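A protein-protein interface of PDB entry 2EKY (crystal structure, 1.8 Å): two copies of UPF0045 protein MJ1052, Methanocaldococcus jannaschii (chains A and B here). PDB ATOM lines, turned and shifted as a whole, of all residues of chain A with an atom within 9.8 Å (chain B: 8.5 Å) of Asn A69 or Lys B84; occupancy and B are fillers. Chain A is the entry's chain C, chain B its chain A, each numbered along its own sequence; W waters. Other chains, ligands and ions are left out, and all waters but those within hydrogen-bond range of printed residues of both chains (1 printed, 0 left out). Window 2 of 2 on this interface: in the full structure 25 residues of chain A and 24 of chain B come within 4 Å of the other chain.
NE of Arg B5 lies within salt-bridge range of OE2 of Glu B82, at 2.7 Å.
The backbone carbonyl oxygen (O) of Lys A61 lies within hydrogen-bond range of the side-chain hydroxyl (OG) of Ser A65, at 2.8 Å.
The backbone carbonyl oxygen of Arg A73 is in hydrogen-bond range of the backbone NH of Leu A16.
The side-chain carboxylate of Asp B85 is in salt-bridge range of the guanidinium group of Arg B83, 2.8 Å away.
The backbone carbonyl oxygen (O) of Ser A65 sits close to the side-chain amide oxygen (OD1) of Asn A69, at 3.3 Å.
The backbone carbonyl oxygen (O) of Asp B81 sits at hydrogen-bond distance from the side-chain amide nitrogen (ND2) of Asn B88.
The backbone NH (N) of Lys B84 lies within hydrogen-bond range of the backbone carbonyl oxygen (O) of Asp A72.
The backbone carbonyl oxygen (O) of Glu B82 lies within hydrogen-bond range of the backbone NH (N) of Val A74.
O of Val A71 sits close to NZ of Lys B84, 3.1 Å away.
The side-chain carboxylate (OD2) of Asp B81 lies within salt-bridge range of the guanidinium group (NH2) of Arg A73, 2.8 Å away.
The guanidinium group of Arg B5 sits at hydrogen-bond distance from the side-chain hydroxyl of Ser A65, at 2.7 Å.
The side-chain amino group (NZ) of Lys B84 sits at hydrogen-bond distance from the backbone carbonyl oxygen (O) of Leu A68, at 3.0 Å.
The side-chain carboxylate (OE1) of Glu B82 lies within hydrogen-bond range of a ring nitrogen (NE2) of His A64.
The side-chain amino group (NZ) of Lys B84 is in hydrogen-bond range of the backbone carbonyl oxygen (O) of Asn A69 (3.3 Å).
The guanidinium group of Arg B83 sits close to the guanidinium group of Arg A73, 3.4 Å away.
Among the printed residues, pairs that only touch across the chains: Lys A61 with Arg B5, His A64 with Arg B5, Leu A68 with Glu B82, Asp A72 with Arg B83, Asp A72 with Asp B85, Arg A73 with Glu B82 and Val A74 with Asp B81.
No position is printed for both chains.
Of the 16 pairs that touch across the chains among the printed residues, none has its exchanged pair printed and touching as well.
Water W1 lies within hydrogen-bond range of the guanidinium group of Arg B5 (3.5 Å) and the side-chain hydroxyl of Ser A65 (3.5 Å).
Along chain B the printed residues that touch a printed residue of chain A span positions 5 to 85.
Of the 21 printed residues of chain A, 9 touch a printed residue of chain B.
Hydrophobic or aromatic side chains of chain A that line the printed part of chain B: His A64 and Leu A68.
Among the printed residues, 16 pairs touch across the chains.
Among the printed residues, Asp or Glu carboxylates within 4 Å of a Lys or Arg side-chain nitrogen of the other chain: Arg A73 with Asp B81 (2.8 Å).
Asn A69 touches one residue of chain B.
Of chain A, only Leu A68 (3.0 Å), Asn A69 (3.3 Å), Val A71 (2.9 Å) and Asp A72 (2.9 Å) come within 4 Å of Lys B84.
Asp B85 touches one residue of chain A.
Printed residues of chain B within 4 Å of Leu A68: Glu B82 and Lys B84.
Of the printed residues of chain B, Ser A65 touches Arg B5 (2.7 Å).
The nearest residue of chain B that does not touch Asn A69 is Arg B5 (7.0 Å).
The nearest residue of chain A that does not touch Lys B84 is Asp A70 (4.3 Å).
The nearest printed residue of chain A that does not touch Glu B82 is Asp A72 (4.2 Å).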
ATOM      1  N   ILE A  13     -25.296 -30.857 -19.520  1.00  0.00           N
ATOM      2  CA  ILE A  13     -24.470 -29.661 -19.445  1.00  0.00           C
ATOM      3  C   ILE A  13     -24.083 -29.464 -17.991  1.00  0.00           C
ATOM      4  O   ILE A  13     -24.945 -29.412 -17.113  1.00  0.00           O
ATOM      5  CB  ILE A  13     -25.237 -28.437 -19.956  1.00  0.00           C
ATOM      6  CG1 ILE A  13     -25.635 -28.663 -21.416  1.00  0.00           C
ATOM      7  CG2 ILE A  13     -24.378 -27.185 -19.825  1.00  0.00           C
ATOM      8  CD1 ILE A  13     -26.618 -27.657 -21.934  1.00  0.00           C
ATOM      9  N   PRO A  15     -21.940 -26.958 -15.463  1.00  0.00           N
ATOM     10  CA  PRO A  15     -21.155 -25.735 -15.280  1.00  0.00           C
ATOM     11  C   PRO A  15     -20.126 -25.994 -14.179  1.00  0.00           C
ATOM     12  O   PRO A  15     -20.441 -26.619 -13.158  1.00  0.00           O
ATOM     13  CB  PRO A  15     -22.206 -24.713 -14.865  1.00  0.00           C
ATOM     14  CG  PRO A  15     -23.159 -25.530 -14.085  1.00  0.00           C
ATOM     15  CD  PRO A  15     -23.292 -26.806 -14.897  1.00  0.00           C
ATOM     16  N   LEU A  16     -18.901 -25.524 -14.384  1.00  0.00           N
ATOM     17  CA  LEU A  16     -17.839 -25.729 -13.405  1.00  0.00           C
ATOM     18  C   LEU A  16     -17.452 -24.429 -12.716  1.00  0.00           C
ATOM     19  O   LEU A  16     -17.678 -23.348 -13.251  1.00  0.00           O
ATOM     20  CB  LEU A  16     -16.595 -26.325 -14.075  1.00  0.00           C
ATOM     21  CG  LEU A  16     -16.595 -27.806 -14.482  1.00  0.00           C
ATOM     22  CD1 LEU A  16     -17.755 -28.101 -15.400  1.00  0.00           C
ATOM     23  CD2 LEU A  16     -15.275 -28.141 -15.174  1.00  0.00           C
ATOM     24  N   LYS A  18     -18.669 -23.153  -9.858  1.00  0.00           N
ATOM     25  CA  LYS A  18     -19.707 -22.525  -9.041  1.00  0.00           C
ATOM     26  C   LYS A  18     -20.217 -23.403  -7.904  1.00  0.00           C
ATOM     27  O   LYS A  18     -21.280 -23.146  -7.340  1.00  0.00           O
ATOM     28  CB  LYS A  18     -20.887 -22.111  -9.927  1.00  0.00           C
ATOM     29  CG  LYS A  18     -20.512 -21.180 -11.073  1.00  0.00           C
ATOM     30  CD  LYS A  18     -19.854 -19.906 -10.561  1.00  0.00           C
ATOM     31  CE  LYS A  18     -19.555 -18.951 -11.702  1.00  0.00           C
ATOM     32  NZ  LYS A  18     -18.912 -17.704 -11.213  1.00  0.00           N
ATOM     33  N   TYR A  25     -28.393 -22.736 -13.586  1.00  0.00           N
ATOM     34  CA  TYR A  25     -27.789 -22.621 -14.911  1.00  0.00           C
ATOM     35  C   TYR A  25     -28.391 -23.662 -15.849  1.00  0.00           C
ATOM     36  O   TYR A  25     -28.758 -23.353 -16.984  1.00  0.00           O
ATOM     37  CB  TYR A  25     -26.275 -22.843 -14.833  1.00  0.00           C
ATOM     38  CG  TYR A  25     -25.561 -21.929 -13.863  1.00  0.00           C
ATOM     39  CD1 TYR A  25     -25.455 -20.561 -14.113  1.00  0.00           C
ATOM     40  CD2 TYR A  25     -25.005 -22.430 -12.687  1.00  0.00           C
ATOM     41  CE1 TYR A  25     -24.815 -19.716 -13.218  1.00  0.00           C
ATOM     42  CE2 TYR A  25     -24.362 -21.589 -11.783  1.00  0.00           C
ATOM     43  CZ  TYR A  25     -24.271 -20.236 -12.055  1.00  0.00           C
ATOM     44  OH  TYR A  25     -23.643 -19.400 -11.164  1.00  0.00           O
ATOM     45  N   LYS A  28     -31.732 -22.894 -17.384  1.00  0.00           N
ATOM     46  CA  LYS A  28     -31.645 -21.974 -18.512  1.00  0.00           C
ATOM     47  C   LYS A  28     -31.309 -22.710 -19.801  1.00  0.00           C
ATOM     48  O   LYS A  28     -31.854 -22.403 -20.859  1.00  0.00           O
ATOM     49  CB  LYS A  28     -30.584 -20.900 -18.257  1.00  0.00           C
ATOM     50  CG  LYS A  28     -30.926 -19.928 -17.146  1.00  0.00           C
ATOM     51  CD  LYS A  28     -29.866 -18.841 -17.028  1.00  0.00           C
ATOM     52  CE  LYS A  28     -29.758 -18.035 -18.315  1.00  0.00           C
ATOM     53  NZ  LYS A  28     -28.746 -16.949 -18.214  1.00  0.00           N
ATOM     54  N   ALA A  29     -30.407 -23.680 -19.707  1.00  0.00           N
ATOM     55  CA  ALA A  29     -29.999 -24.455 -20.871  1.00  0.00           C
ATOM     56  C   ALA A  29     -31.176 -25.244 -21.434  1.00  0.00           C
ATOM     57  O   ALA A  29     -31.367 -25.311 -22.649  1.00  0.00           O
ATOM     58  CB  ALA A  29     -28.859 -25.402 -20.495  1.00  0.00           C
ATOM     59  N   LYS A  61     -25.414 -26.580 -29.077  1.00  0.00           N
ATOM     60  CA  LYS A  61     -24.473 -25.467 -29.038  1.00  0.00           C
ATOM     61  C   LYS A  61     -25.048 -24.296 -28.238  1.00  0.00           C
ATOM     62  O   LYS A  61     -24.358 -23.720 -27.394  1.00  0.00           O
ATOM     63  CB  LYS A  61     -24.132 -24.998 -30.458  1.00  0.00           C
ATOM     64  CG  LYS A  61     -23.174 -23.807 -30.495  1.00  0.00           C
ATOM     65  CD  LYS A  61     -23.035 -23.227 -31.894  1.00  0.00           C
ATOM     66  CE  LYS A  61     -22.101 -22.020 -31.883  1.00  0.00           C
ATOM     67  NZ  LYS A  61     -22.032 -21.347 -33.211  1.00  0.00           N
ATOM     68  N   GLU A  62     -26.310 -23.949 -28.479  1.00  0.00           N
ATOM     69  CA  GLU A  62     -26.909 -22.825 -27.752  1.00  0.00           C
ATOM     70  C   GLU A  62     -27.060 -23.094 -26.255  1.00  0.00           C
ATOM     71  O   GLU A  62     -26.766 -22.226 -25.431  1.00  0.00           O
ATOM     72  CB  GLU A  62     -28.277 -22.444 -28.335  1.00  0.00           C
ATOM     73  CG  GLU A  62     -28.877 -21.214 -27.640  1.00  0.00           C
ATOM     74  CD  GLU A  62     -30.223 -20.781 -28.204  1.00  0.00           C
ATOM     75  OE1 GLU A  62     -30.705 -21.400 -29.173  1.00  0.00           O
ATOM     76  OE2 GLU A  62     -30.800 -19.810 -27.669  1.00  0.00           O
ATOM     77  N   ALA A  63     -27.526 -24.286 -25.899  1.00  0.00           N
ATOM     78  CA  ALA A  63     -27.697 -24.635 -24.496  1.00  0.00           C
ATOM     79  C   ALA A  63     -26.347 -24.527 -23.789  1.00  0.00           C
ATOM     80  O   ALA A  63     -26.253 -23.988 -22.683  1.00  0.00           O
ATOM     81  CB  ALA A  63     -28.246 -26.052 -24.371  1.00  0.00           C
ATOM     82  N   HIS A  64     -25.310 -25.046 -24.440  1.00  0.00           N
ATOM     83  CA  HIS A  64     -23.950 -25.010 -23.915  1.00  0.00           C
ATOM     84  C   HIS A  64     -23.501 -23.564 -23.724  1.00  0.00           C
ATOM     85  O   HIS A  64     -23.000 -23.190 -22.665  1.00  0.00           O
ATOM     86  CB  HIS A  64     -23.002 -25.716 -24.888  1.00  0.00           C
ATOM     87  CG  HIS A  64     -21.547 -25.490 -24.603  1.00  0.00           C
ATOM     88  ND1 HIS A  64     -20.873 -26.137 -23.587  1.00  0.00           N
ATOM     89  CD2 HIS A  64     -20.635 -24.698 -25.214  1.00  0.00           C
ATOM     90  CE1 HIS A  64     -19.609 -25.753 -23.588  1.00  0.00           C
ATOM     91  NE2 HIS A  64     -19.437 -24.879 -24.565  1.00  0.00           N
ATOM     92  N   SER A  65     -23.689 -22.756 -24.766  1.00  0.00           N
ATOM     93  CA  SER A  65     -23.289 -21.353 -24.745  1.00  0.00           C
ATOM     94  C   SER A  65     -24.067 -20.513 -23.741  1.00  0.00           C
ATOM     95  O   SER A  65     -23.527 -19.574 -23.149  1.00  0.00           O
ATOM     96  CB  SER A  65     -23.438 -20.759 -26.148  1.00  0.00           C
ATOM     97  OG  SER A  65     -22.678 -21.496 -27.089  1.00  0.00           O
ATOM     98  N   THR A  66     -25.340 -20.844 -23.554  1.00  0.00           N
ATOM     99  CA  THR A  66     -26.181 -20.117 -22.611  1.00  0.00           C
ATOM    100  C   THR A  66     -25.615 -20.215 -21.201  1.00  0.00           C
ATOM    101  O   THR A  66     -25.595 -19.232 -20.459  1.00  0.00           O
ATOM    102  CB  THR A  66     -27.625 -20.665 -22.634  1.00  0.00           C
ATOM    103  OG1 THR A  66     -28.191 -20.430 -23.927  1.00  0.00           O
ATOM    104  CG2 THR A  66     -28.487 -19.982 -21.585  1.00  0.00           C
ATOM    105  N   VAL A  67     -25.138 -21.399 -20.836  1.00  0.00           N
ATOM    106  CA  VAL A  67     -24.569 -21.592 -19.511  1.00  0.00           C
ATOM    107  C   VAL A  67     -23.219 -20.880 -19.401  1.00  0.00           C
ATOM    108  O   VAL A  67     -22.933 -20.214 -18.404  1.00  0.00           O
ATOM    109  CB  VAL A  67     -24.394 -23.102 -19.198  1.00  0.00           C
ATOM    110  CG1 VAL A  67     -23.669 -23.281 -17.878  1.00  0.00           C
ATOM    111  CG2 VAL A  67     -25.765 -23.778 -19.137  1.00  0.00           C
ATOM    112  N   LEU A  68     -22.399 -21.012 -20.436  1.00  0.00           N
ATOM    113  CA  LEU A  68     -21.078 -20.391 -20.445  1.00  0.00           C
ATOM    114  C   LEU A  68     -21.157 -18.876 -20.267  1.00  0.00           C
ATOM    115  O   LEU A  68     -20.176 -18.231 -19.894  1.00  0.00           O
ATOM    116  CB  LEU A  68     -20.349 -20.728 -21.748  1.00  0.00           C
ATOM    117  CG  LEU A  68     -18.892 -20.271 -21.847  1.00  0.00           C
ATOM    118  CD1 LEU A  68     -18.069 -20.892 -20.721  1.00  0.00           C
ATOM    119  CD2 LEU A  68     -18.334 -20.666 -23.200  1.00  0.00           C
ATOM    120  N   ASN A  69     -22.325 -18.306 -20.530  1.00  0.00           N
ATOM    121  CA  ASN A  69     -22.500 -16.869 -20.373  1.00  0.00           C
ATOM    122  C   ASN A  69     -22.442 -16.420 -18.915  1.00  0.00           C
ATOM    123  O   ASN A  69     -22.057 -15.287 -18.627  1.00  0.00           O
ATOM    124  CB  ASN A  69     -23.831 -16.425 -20.975  1.00  0.00           C
ATOM    125  CG  ASN A  69     -23.655 -15.709 -22.289  1.00  0.00           C
ATOM    126  OD1 ASN A  69     -23.247 -16.305 -23.288  1.00  0.00           O
ATOM    127  ND2 ASN A  69     -23.945 -14.411 -22.294  1.00  0.00           N
ATOM    128  N   ASP A  70     -22.817 -17.306 -17.996  1.00  0.00           N
ATOM    129  CA  ASP A  70     -22.825 -16.960 -16.579  1.00  0.00           C
ATOM    130  C   ASP A  70     -21.754 -17.645 -15.733  1.00  0.00           C
ATOM    131  O   ASP A  70     -21.654 -17.390 -14.532  1.00  0.00           O
ATOM    132  CB  ASP A  70     -24.204 -17.252 -15.980  1.00  0.00           C
ATOM    133  CG  ASP A  70     -25.320 -16.546 -16.719  1.00  0.00           C
ATOM    134  OD1 ASP A  70     -25.201 -15.322 -16.941  1.00  0.00           O
ATOM    135  OD2 ASP A  70     -26.317 -17.210 -17.073  1.00  0.00           O
ATOM    136  N   VAL A  71     -20.963 -18.520 -16.345  1.00  0.00           N
ATOM    137  CA  VAL A  71     -19.904 -19.201 -15.611  1.00  0.00           C
ATOM    138  C   VAL A  71     -18.612 -19.138 -16.420  1.00  0.00           C
ATOM    139  O   VAL A  71     -18.621 -18.714 -17.577  1.00  0.00           O
ATOM    140  CB  VAL A  71     -20.275 -20.673 -15.319  1.00  0.00           C
ATOM    141  CG1 VAL A  71     -21.618 -20.733 -14.588  1.00  0.00           C
ATOM    142  CG2 VAL A  71     -20.335 -21.468 -16.615  1.00  0.00           C
ATOM    143  N   ASP A  72     -17.502 -19.551 -15.819  1.00  0.00           N
ATOM    144  CA  ASP A  72     -16.225 -19.501 -16.516  1.00  0.00           C
ATOM    145  C   ASP A  72     -15.895 -20.750 -17.318  1.00  0.00           C
ATOM    146  O   ASP A  72     -15.093 -20.695 -18.248  1.00  0.00           O
ATOM    147  CB  ASP A  72     -15.090 -19.224 -15.528  1.00  0.00           C
ATOM    148  CG  ASP A  72     -15.174 -17.837 -14.927  1.00  0.00           C
ATOM    149  OD1 ASP A  72     -15.427 -16.883 -15.688  1.00  0.00           O
ATOM    150  OD2 ASP A  72     -14.982 -17.699 -13.702  1.00  0.00           O
ATOM    151  N   ARG A  73     -16.513 -21.871 -16.971  1.00  0.00           N
ATOM    152  CA  ARG A  73     -16.226 -23.113 -17.675  1.00  0.00           C
ATOM    153  C   ARG A  73     -17.430 -24.043 -17.706  1.00  0.00           C
ATOM    154  O   ARG A  73     -18.193 -24.119 -16.741  1.00  0.00           O
ATOM    155  CB  ARG A  73     -15.048 -23.801 -17.000  1.00  0.00           C
ATOM    156  CG  ARG A  73     -14.547 -25.048 -17.693  1.00  0.00           C
ATOM    157  CD  ARG A  73     -13.318 -25.527 -16.965  1.00  0.00           C
ATOM    158  NE  ARG A  73     -12.587 -26.552 -17.702  1.00  0.00           N
ATOM    159  CZ  ARG A  73     -11.437 -27.068 -17.281  1.00  0.00           C
ATOM    160  NH1 ARG A  73     -10.913 -26.648 -16.137  1.00  0.00           N
ATOM    161  NH2 ARG A  73     -10.803 -27.979 -18.006  1.00  0.00           N
ATOM    162  N   VAL A  74     -17.589 -24.754 -18.820  1.00  0.00           N
ATOM    163  CA  VAL A  74     -18.714 -25.669 -18.998  1.00  0.00           C
ATOM    164  C   VAL A  74     -18.294 -26.936 -19.737  1.00  0.00           C
ATOM    165  O   VAL A  74     -17.612 -26.861 -20.754  1.00  0.00           O
ATOM    166  CB  VAL A  74     -19.847 -24.996 -19.830  1.00  0.00           C
ATOM    167  CG1 VAL A  74     -21.012 -25.958 -20.003  1.00  0.00           C
ATOM    168  CG2 VAL A  74     -20.306 -23.711 -19.148  1.00  0.00           C
ATOM    169  N   ARG B   5     -13.479 -19.752 -31.798  1.00  0.00           N
ATOM    170  CA  ARG B   5     -13.991 -20.089 -30.481  1.00  0.00           C
ATOM    171  C   ARG B   5     -13.414 -21.468 -30.173  1.00  0.00           C
ATOM    172  O   ARG B   5     -14.065 -22.493 -30.377  1.00  0.00           O
ATOM    173  CB  ARG B   5     -15.516 -20.127 -30.513  1.00  0.00           C
ATOM    174  CG  ARG B   5     -16.150 -20.379 -29.173  1.00  0.00           C
ATOM    175  CD  ARG B   5     -17.654 -20.238 -29.249  1.00  0.00           C
ATOM    176  NE  ARG B   5     -18.279 -20.801 -28.061  1.00  0.00           N
ATOM    177  CZ  ARG B   5     -19.588 -20.882 -27.866  1.00  0.00           C
ATOM    178  NH1 ARG B   5     -20.435 -20.429 -28.785  1.00  0.00           N
ATOM    179  NH2 ARG B   5     -20.048 -21.441 -26.756  1.00  0.00           N
ATOM    180  N   LYS B   6     -12.178 -21.479 -29.693  1.00  0.00           N
ATOM    181  CA  LYS B   6     -11.476 -22.724 -29.401  1.00  0.00           C
ATOM    182  C   LYS B   6     -11.950 -23.498 -28.182  1.00  0.00           C
ATOM    183  O   LYS B   6     -12.187 -22.930 -27.117  1.00  0.00           O
ATOM    184  CB  LYS B   6      -9.973 -22.457 -29.266  1.00  0.00           C
ATOM    185  CG  LYS B   6      -9.171 -23.690 -28.890  1.00  0.00           C
ATOM    186  CD  LYS B   6      -7.674 -23.429 -28.920  1.00  0.00           C
ATOM    187  CE  LYS B   6      -7.198 -23.125 -30.329  1.00  0.00           C
ATOM    188  NZ  LYS B   6      -5.719 -23.013 -30.389  1.00  0.00           N
ATOM    189  N   ASP B  81     -15.298 -29.204 -23.721  1.00  0.00           N
ATOM    190  CA  ASP B  81     -14.809 -28.544 -22.518  1.00  0.00           C
ATOM    191  C   ASP B  81     -14.432 -27.136 -22.977  1.00  0.00           C
ATOM    192  O   ASP B  81     -13.460 -26.955 -23.704  1.00  0.00           O
ATOM    193  CB  ASP B  81     -13.587 -29.279 -21.946  1.00  0.00           C
ATOM    194  CG  ASP B  81     -12.923 -28.517 -20.797  1.00  0.00           C
ATOM    195  OD1 ASP B  81     -13.596 -27.681 -20.162  1.00  0.00           O
ATOM    196  OD2 ASP B  81     -11.730 -28.765 -20.523  1.00  0.00           O
ATOM    197  N   GLU B  82     -15.228 -26.146 -22.585  1.00  0.00           N
ATOM    198  CA  GLU B  82     -14.953 -24.768 -22.975  1.00  0.00           C
ATOM    199  C   GLU B  82     -14.864 -23.858 -21.759  1.00  0.00           C
ATOM    200  O   GLU B  82     -15.681 -23.945 -20.845  1.00  0.00           O
ATOM    201  CB  GLU B  82     -16.039 -24.246 -23.925  1.00  0.00           C
ATOM    202  CG  GLU B  82     -15.837 -22.794 -24.358  1.00  0.00           C
ATOM    203  CD  GLU B  82     -16.758 -22.374 -25.495  1.00  0.00           C
ATOM    204  OE1 GLU B  82     -17.827 -22.996 -25.668  1.00  0.00           O
ATOM    205  OE2 GLU B  82     -16.419 -21.402 -26.206  1.00  0.00           O
ATOM    206  N   ARG B  83     -13.863 -22.988 -21.753  1.00  0.00           N
ATOM    207  CA  ARG B  83     -13.685 -22.042 -20.660  1.00  0.00           C
ATOM    208  C   ARG B  83     -13.382 -20.671 -21.257  1.00  0.00           C
ATOM    209  O   ARG B  83     -12.868 -20.576 -22.373  1.00  0.00           O
ATOM    210  CB  ARG B  83     -12.556 -22.504 -19.738  1.00  0.00           C
ATOM    211  CG  ARG B  83     -11.187 -22.568 -20.382  1.00  0.00           C
ATOM    212  CD  ARG B  83     -10.214 -23.325 -19.478  1.00  0.00           C
ATOM    213  NE  ARG B  83     -10.169 -22.765 -18.128  1.00  0.00           N
ATOM    214  CZ  ARG B  83      -9.458 -23.276 -17.126  1.00  0.00           C
ATOM    215  NH1 ARG B  83      -8.723 -24.365 -17.316  1.00  0.00           N
ATOM    216  NH2 ARG B  83      -9.486 -22.703 -15.930  1.00  0.00           N
ATOM    217  N   LYS B  84     -13.720 -19.610 -20.527  1.00  0.00           N
ATOM    218  CA  LYS B  84     -13.491 -18.256 -21.019  1.00  0.00           C
ATOM    219  C   LYS B  84     -12.513 -17.487 -20.142  1.00  0.00           C
ATOM    220  O   LYS B  84     -12.198 -16.330 -20.417  1.00  0.00           O
ATOM    221  CB  LYS B  84     -14.820 -17.495 -21.099  1.00  0.00           C
ATOM    222  CG  LYS B  84     -15.470 -17.235 -19.743  1.00  0.00           C
ATOM    223  CD  LYS B  84     -16.871 -16.657 -19.887  1.00  0.00           C
ATOM    224  CE  LYS B  84     -17.416 -16.220 -18.532  1.00  0.00           C
ATOM    225  NZ  LYS B  84     -18.843 -15.813 -18.608  1.00  0.00           N
ATOM    226  N   ASP B  85     -12.032 -18.129 -19.085  1.00  0.00           N
ATOM    227  CA  ASP B  85     -11.087 -17.483 -18.180  1.00  0.00           C
ATOM    228  C   ASP B  85      -9.641 -17.691 -18.641  1.00  0.00           C
ATOM    229  O   ASP B  85      -8.744 -16.923 -18.280  1.00  0.00           O
ATOM    230  CB  ASP B  85     -11.275 -18.025 -16.762  1.00  0.00           C
ATOM    231  CG  ASP B  85     -11.017 -19.515 -16.665  1.00  0.00           C
ATOM    232  OD1 ASP B  85     -11.411 -20.260 -17.592  1.00  0.00           O
ATOM    233  OD2 ASP B  85     -10.431 -19.942 -15.650  1.00  0.00           O
ATOM    234  N   LYS B  86      -9.425 -18.726 -19.449  1.00  0.00           N
ATOM    235  CA  LYS B  86      -8.095 -19.045 -19.961  1.00  0.00           C
ATOM    236  C   LYS B  86      -8.190 -19.690 -21.335  1.00  0.00           C
ATOM    237  O   LYS B  86      -9.250 -20.178 -21.734  1.00  0.00           O
ATOM    238  CB  LYS B  86      -7.385 -20.047 -19.048  1.00  0.00           C
ATOM    239  CG  LYS B  86      -7.277 -19.670 -17.590  1.00  0.00           C
ATOM    240  CD  LYS B  86      -6.668 -20.830 -16.816  1.00  0.00           C
ATOM    241  CE  LYS B  86      -6.462 -20.485 -15.358  1.00  0.00           C
ATOM    242  NZ  LYS B  86      -5.722 -21.564 -14.651  1.00  0.00           N
ATOM    243  N   GLU B  87      -7.070 -19.692 -22.047  1.00  0.00           N
ATOM    244  CA  GLU B  87      -6.980 -20.326 -23.356  1.00  0.00           C
ATOM    245  C   GLU B  87      -7.008 -21.818 -23.042  1.00  0.00           C
ATOM    246  O   GLU B  87      -6.326 -22.262 -22.120  1.00  0.00           O
ATOM    247  CB  GLU B  87      -5.655 -19.958 -24.023  1.00  0.00           C
ATOM    248  CG  GLU B  87      -5.303 -20.790 -25.252  1.00  0.00           C
ATOM    249  CD  GLU B  87      -3.895 -20.520 -25.746  1.00  0.00           C
ATOM    250  OE1 GLU B  87      -2.955 -20.595 -24.927  1.00  0.00           O
ATOM    251  OE2 GLU B  87      -3.726 -20.239 -26.952  1.00  0.00           O
ATOM    252  N   ASN B  88      -7.787 -22.588 -23.795  1.00  0.00           N
ATOM    253  CA  ASN B  88      -7.887 -24.021 -23.548  1.00  0.00           C
ATOM    254  C   ASN B  88      -7.363 -24.823 -24.734  1.00  0.00           C
ATOM    255  O   ASN B  88      -7.851 -24.684 -25.853  1.00  0.00           O
ATOM    256  CB  ASN B  88      -9.349 -24.390 -23.249  1.00  0.00           C
ATOM    257  CG  ASN B  88      -9.498 -25.785 -22.659  1.00  0.00           C
ATOM    258  OD1 ASN B  88      -8.572 -26.315 -22.053  1.00  0.00           O
ATOM    259  ND2 ASN B  88     -10.682 -26.371 -22.812  1.00  0.00           N
HETATM  260  O   HOH W   1     -23.642 -19.635 -29.863  1.00  0.00           O
